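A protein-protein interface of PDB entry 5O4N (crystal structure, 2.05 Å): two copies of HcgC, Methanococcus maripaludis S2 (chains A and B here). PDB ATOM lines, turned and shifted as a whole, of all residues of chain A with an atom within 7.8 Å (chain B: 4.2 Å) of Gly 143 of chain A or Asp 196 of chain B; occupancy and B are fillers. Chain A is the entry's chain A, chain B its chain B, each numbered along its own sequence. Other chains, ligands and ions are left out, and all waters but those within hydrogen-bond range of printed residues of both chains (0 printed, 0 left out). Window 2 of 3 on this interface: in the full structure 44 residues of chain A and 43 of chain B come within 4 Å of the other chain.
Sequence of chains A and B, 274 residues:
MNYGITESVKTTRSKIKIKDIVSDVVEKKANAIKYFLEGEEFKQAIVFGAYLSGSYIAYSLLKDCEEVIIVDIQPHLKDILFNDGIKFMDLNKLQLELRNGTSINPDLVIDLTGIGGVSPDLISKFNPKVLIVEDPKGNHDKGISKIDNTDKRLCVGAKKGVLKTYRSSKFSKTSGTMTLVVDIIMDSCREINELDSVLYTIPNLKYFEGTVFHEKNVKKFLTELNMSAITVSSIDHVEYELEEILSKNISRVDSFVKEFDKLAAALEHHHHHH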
ATOM      1  N   ILE A 115     -26.659   3.945  27.537  1.00  0.00           N
ATOM      2  CA  ILE A 115     -25.522   4.257  26.655  1.00  0.00           C
ATOM      3  C   ILE A 115     -25.525   5.713  26.145  1.00  0.00           C
ATOM      4  O   ILE A 115     -26.481   6.154  25.499  1.00  0.00           O
ATOM      5  CB  ILE A 115     -25.388   3.234  25.478  1.00  0.00           C
ATOM      6  CG1 ILE A 115     -25.106   1.800  26.004  1.00  0.00           C
ATOM      7  CG2 ILE A 115     -24.262   3.657  24.531  1.00  0.00           C
ATOM      8  CD1 ILE A 115     -25.611   0.690  25.072  1.00  0.00           C
ATOM      9  N   HIS A 140     -22.563 -10.514  27.930  1.00  0.00           N
ATOM     10  CA  HIS A 140     -21.221 -10.021  27.616  1.00  0.00           C
ATOM     11  C   HIS A 140     -20.845  -9.716  26.167  1.00  0.00           C
ATOM     12  O   HIS A 140     -20.953 -10.537  25.258  1.00  0.00           O
ATOM     13  CB  HIS A 140     -20.130 -10.910  28.175  1.00  0.00           C
ATOM     14  CG  HIS A 140     -18.818 -10.181  28.275  1.00  0.00           C
ATOM     15  ND1 HIS A 140     -18.665  -9.091  29.107  1.00  0.00           N
ATOM     16  CD2 HIS A 140     -17.659 -10.397  27.623  1.00  0.00           C
ATOM     17  CE1 HIS A 140     -17.421  -8.686  28.942  1.00  0.00           C
ATOM     18  NE2 HIS A 140     -16.787  -9.437  28.049  1.00  0.00           N
ATOM     19  N   ASP A 141     -20.362  -8.484  26.011  1.00  0.00           N
ATOM     20  CA  ASP A 141     -19.867  -7.884  24.768  1.00  0.00           C
ATOM     21  C   ASP A 141     -18.815  -6.829  25.179  1.00  0.00           C
ATOM     22  O   ASP A 141     -19.128  -5.889  25.911  1.00  0.00           O
ATOM     23  CB  ASP A 141     -21.021  -7.224  24.006  1.00  0.00           C
ATOM     24  CG  ASP A 141     -20.608  -6.613  22.682  1.00  0.00           C
ATOM     25  OD1 ASP A 141     -20.183  -5.429  22.678  1.00  0.00           O
ATOM     26  OD2 ASP A 141     -20.718  -7.308  21.646  1.00  0.00           O
ATOM     27  N   LYS A 142     -17.592  -6.978  24.718  1.00  0.00           N
ATOM     28  CA  LYS A 142     -16.492  -6.054  25.038  1.00  0.00           C
ATOM     29  C   LYS A 142     -16.754  -4.585  24.656  1.00  0.00           C
ATOM     30  O   LYS A 142     -16.504  -3.703  25.472  1.00  0.00           O
ATOM     31  CB  LYS A 142     -15.183  -6.541  24.408  1.00  0.00           C
ATOM     32  CG  LYS A 142     -14.628  -7.795  25.073  1.00  0.00           C
ATOM     33  CD  LYS A 142     -13.404  -8.303  24.306  1.00  0.00           C
ATOM     34  CE  LYS A 142     -12.786  -9.568  24.853  1.00  0.00           C
ATOM     35  NZ  LYS A 142     -13.242 -10.794  24.135  1.00  0.00           N
ATOM     36  N   GLY A 143     -17.248  -4.353  23.430  1.00  0.00           N
ATOM     37  CA  GLY A 143     -17.569  -3.026  22.907  1.00  0.00           C
ATOM     38  C   GLY A 143     -18.599  -2.296  23.747  1.00  0.00           C
ATOM     39  O   GLY A 143     -18.450  -1.111  24.042  1.00  0.00           O
ATOM     40  N   ILE A 144     -19.649  -2.998  24.154  1.00  0.00           N
ATOM     41  CA  ILE A 144     -20.697  -2.401  24.980  1.00  0.00           C
ATOM     42  C   ILE A 144     -20.189  -2.136  26.409  1.00  0.00           C
ATOM     43  O   ILE A 144     -20.510  -1.105  26.984  1.00  0.00           O
ATOM     44  CB  ILE A 144     -21.980  -3.275  24.952  1.00  0.00           C
ATOM     45  CG1 ILE A 144     -22.587  -3.249  23.529  1.00  0.00           C
ATOM     46  CG2 ILE A 144     -23.004  -2.764  25.971  1.00  0.00           C
ATOM     47  CD1 ILE A 144     -23.600  -4.341  23.226  1.00  0.00           C
ATOM     48  N   SER A 145     -19.420  -3.069  26.985  1.00  0.00           N
ATOM     49  CA  SER A 145     -18.865  -2.918  28.353  1.00  0.00           C
ATOM     50  C   SER A 145     -17.916  -1.712  28.440  1.00  0.00           C
ATOM     51  O   SER A 145     -17.916  -1.007  29.442  1.00  0.00           O
ATOM     52  CB  SER A 145     -18.157  -4.197  28.825  1.00  0.00           C
ATOM     53  OG  SER A 145     -17.444  -4.905  27.832  1.00  0.00           O
ATOM     54  N   LYS A 146     -17.138  -1.476  27.385  1.00  0.00           N
ATOM     55  CA  LYS A 146     -16.194  -0.351  27.332  1.00  0.00           C
ATOM     56  C   LYS A 146     -16.905   1.014  27.406  1.00  0.00           C
ATOM     57  O   LYS A 146     -16.442   1.885  28.136  1.00  0.00           O
ATOM     58  CB  LYS A 146     -15.337  -0.441  26.058  1.00  0.00           C
ATOM     59  CG  LYS A 146     -14.039   0.309  26.110  1.00  0.00           C
ATOM     60  CD  LYS A 146     -13.307   0.208  24.744  1.00  0.00           C
ATOM     61  CE  LYS A 146     -12.382   1.335  24.296  1.00  0.00           C
ATOM     62  NZ  LYS A 146     -11.839   2.213  25.370  1.00  0.00           N
ATOM     63  N   ILE A 147     -18.009   1.198  26.663  1.00  0.00           N
ATOM     64  CA  ILE A 147     -18.735   2.476  26.651  1.00  0.00           C
ATOM     65  C   ILE A 147     -19.636   2.674  27.884  1.00  0.00           C
ATOM     66  O   ILE A 147     -19.976   3.809  28.211  1.00  0.00           O
ATOM     67  CB  ILE A 147     -19.510   2.656  25.305  1.00  0.00           C
ATOM     68  CG1 ILE A 147     -19.775   4.153  25.021  1.00  0.00           C
ATOM     69  CG2 ILE A 147     -20.813   1.843  25.250  1.00  0.00           C
ATOM     70  CD1 ILE A 147     -20.039   4.492  23.593  1.00  0.00           C
ATOM     71  N   ASP A 148     -20.020   1.585  28.558  1.00  0.00           N
ATOM     72  CA  ASP A 148     -20.873   1.645  29.735  1.00  0.00           C
ATOM     73  C   ASP A 148     -20.188   2.253  30.970  1.00  0.00           C
ATOM     74  O   ASP A 148     -19.064   1.882  31.270  1.00  0.00           O
ATOM     75  CB  ASP A 148     -21.374   0.232  30.074  1.00  0.00           C
ATOM     76  CG  ASP A 148     -22.179   0.203  31.358  1.00  0.00           C
ATOM     77  OD1 ASP A 148     -23.275   0.790  31.377  1.00  0.00           O
ATOM     78  OD2 ASP A 148     -21.641  -0.281  32.391  1.00  0.00           O
ATOM     79  N   LYS A 173     -27.844  -8.484  23.710  1.00  0.00           N
ATOM     80  CA  LYS A 173     -26.727  -7.546  23.866  1.00  0.00           C
ATOM     81  C   LYS A 173     -26.965  -6.438  24.851  1.00  0.00           C
ATOM     82  O   LYS A 173     -26.010  -5.932  25.394  1.00  0.00           O
ATOM     83  CB  LYS A 173     -26.356  -6.965  22.504  1.00  0.00           C
ATOM     84  CG  LYS A 173     -25.711  -7.979  21.594  1.00  0.00           C
ATOM     85  CD  LYS A 173     -24.223  -8.168  21.995  1.00  0.00           C
ATOM     86  CE  LYS A 173     -23.412  -8.891  20.978  1.00  0.00           C
ATOM     87  NZ  LYS A 173     -22.961  -7.972  19.919  1.00  0.00           N
ATOM     88  N   GLU B 194     -24.008 -11.047  16.636  1.00  0.00           N
ATOM     89  CA  GLU B 194     -22.891 -11.536  17.424  1.00  0.00           C
ATOM     90  C   GLU B 194     -21.609 -10.686  17.218  1.00  0.00           C
ATOM     91  O   GLU B 194     -20.657 -10.907  17.928  1.00  0.00           O
ATOM     92  CB  GLU B 194     -22.624 -13.007  17.116  1.00  0.00           C
ATOM     93  CG  GLU B 194     -23.797 -13.874  17.537  1.00  0.00           C
ATOM     94  CD  GLU B 194     -23.608 -15.371  17.448  1.00  0.00           C
ATOM     95  OE1 GLU B 194     -22.604 -15.813  16.843  1.00  0.00           O
ATOM     96  OE2 GLU B 194     -24.480 -16.104  17.975  1.00  0.00           O
ATOM     97  N   LEU B 195     -21.580  -9.728  16.283  1.00  0.00           N
ATOM     98  CA  LEU B 195     -20.392  -8.898  16.074  1.00  0.00           C
ATOM     99  C   LEU B 195     -20.210  -8.027  17.319  1.00  0.00           C
ATOM    100  O   LEU B 195     -21.195  -7.591  17.927  1.00  0.00           O
ATOM    101  CB  LEU B 195     -20.520  -7.994  14.851  1.00  0.00           C
ATOM    102  CG  LEU B 195     -20.646  -8.677  13.510  1.00  0.00           C
ATOM    103  CD1 LEU B 195     -21.117  -7.682  12.457  1.00  0.00           C
ATOM    104  CD2 LEU B 195     -19.331  -9.357  13.114  1.00  0.00           C
ATOM    105  N   ASP B 196     -18.963  -7.777  17.688  1.00  0.00           N
ATOM    106  CA  ASP B 196     -18.684  -6.966  18.862  1.00  0.00           C
ATOM    107  C   ASP B 196     -19.274  -5.566  18.690  1.00  0.00           C
ATOM    108  O   ASP B 196     -19.225  -5.005  17.597  1.00  0.00           O
ATOM    109  CB  ASP B 196     -17.177  -6.862  19.133  1.00  0.00           C
ATOM    110  CG  ASP B 196     -16.852  -5.983  20.330  1.00  0.00           C
ATOM    111  OD1 ASP B 196     -17.320  -6.309  21.444  1.00  0.00           O
ATOM    112  OD2 ASP B 196     -16.222  -4.907  20.129  1.00  0.00           O
ATOM    113  N   SER B 197     -19.848  -5.024  19.777  1.00  0.00           N
ATOM    114  CA  SER B 197     -20.454  -3.702  19.874  1.00  0.00           C
ATOM    115  C   SER B 197     -21.856  -3.598  19.314  1.00  0.00           C
ATOM    116  O   SER B 197     -22.475  -2.562  19.551  1.00  0.00           O
ATOM    117  CB  SER B 197     -19.534  -2.641  19.250  1.00  0.00           C
ATOM    118  OG  SER B 197     -19.836  -2.380  17.888  1.00  0.00           O
ATOM    119  N   VAL B 198     -22.385  -4.618  18.582  1.00  0.00           N
ATOM    120  CA  VAL B 198     -23.738  -4.555  18.056  1.00  0.00           C
ATOM    121  C   VAL B 198     -24.742  -4.615  19.214  1.00  0.00           C
ATOM    122  O   VAL B 198     -24.612  -5.466  20.064  1.00  0.00           O
ATOM    123  CB  VAL B 198     -24.022  -5.646  16.979  1.00  0.00           C
ATOM    124  CG1 VAL B 198     -25.512  -5.733  16.643  1.00  0.00           C
ATOM    125  CG2 VAL B 198     -23.220  -5.350  15.724  1.00  0.00           C
ATOM    126  N   ASP B 236     -19.601   0.562  17.605  1.00  0.00           N
ATOM    127  CA  ASP B 236     -18.514   0.677  16.636  1.00  0.00           C
ATOM    128  C   ASP B 236     -18.977   0.438  15.208  1.00  0.00           C
ATOM    129  O   ASP B 236     -20.088  -0.011  14.993  1.00  0.00           O
ATOM    130  CB  ASP B 236     -17.387  -0.289  17.023  1.00  0.00           C
ATOM    131  CG  ASP B 236     -16.819  -0.031  18.412  1.00  0.00           C
ATOM    132  OD1 ASP B 236     -16.456   1.142  18.704  1.00  0.00           O
ATOM    133  OD2 ASP B 236     -16.700  -1.005  19.196  1.00  0.00           O
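Among the printed residues, pairs that only touch across the chains: Ile 144 of chain A with Val 198 of chain B and Asp 141 of chain A with Leu 195 of chain B.
OD2 of Asp 141 of chain A lies within salt-bridge range of NZ of Lys 173 of chain A (2.9 Å). The backbone NH of Gly 143 of chain A is in hydrogen-bond range of the side-chain carboxylate of Asp 141 of chain A (3.2 Å). The backbone carbonyl oxygen (O) of Lys 142 of chain A is in hydrogen-bond range of the side-chain hydroxyl (OG) of Ser 145 of chain A, 2.8 Å away. O of Asp 141 of chain A lies within hydrogen-bond range of OG of Ser 145 of chain A (2.7 Å). The side-chain carboxylate (OD1) of Asp 141 of chain A is in hydrogen-bond range of the backbone NH (N) of Ile 144 of chain A (2.9 Å). N of Asp 236 of chain B sits at hydrogen-bond distance from OG of Ser 197 of chain B.
Gly 143 of chain A touches one residue of chain B. Of the printed residues of chain A, Val 198 of chain B touches Ile 144 and Lys 173. Of the printed residues of chain B, Asp 141 of chain A touches Leu 195 (3.8 Å), Asp 196 (3.2 Å) and Ser 197 (2.9 Å). Of the printed residues of chain A, Leu 195 of chain B touches Asp 141 and Lys 173. Asp 236 of chain B touches none of the printed residues of chain A. The nearest printed residue of chain B that does not touch Gly 143 of chain A is Ser 197 of chain B (4.2 Å).
Hydrophobic or aromatic side chains of chain B that line the printed part of chain A: Val 198. Hydrophobic or aromatic side chains of chain A that line the printed part of chain B: Ile 144. Among the printed residues, 8 pairs touch across the chains. Among the printed residues, no Asp or Glu carboxylate lies within 4 Å of a Lys or Arg side-chain nitrogen of the other chain.
NZ of Lys 173 of chain A lies within hydrogen-bond range of O of Leu 195 of chain B (2.7 Å). The side-chain carboxylate (OD1) of Asp 141 of chain A sits close to the side-chain carboxylate (OD1) of Asp 196 of chain B (3.2 Å). NZ of Lys 173 of chain A lies within hydrogen-bond range of O of Val 198 of chain B (3.0 Å). N of Lys 142 of chain A sits at hydrogen-bond distance from OD1 of Asp 196 of chain B (3.4 Å). OD1 of Asp 196 of chain B is in hydrogen-bond range of N of Gly 143 of chain A (2.8 Å). The side-chain carboxylate (OD1) of Asp 141 of chain A is in hydrogen-bond range of the backbone NH (N) of Ser 197 of chain B.
No position is printed for both chains. Of the 8 pairs that touch across the chains among the printed residues, none has its exchanged pair printed and touching as well.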
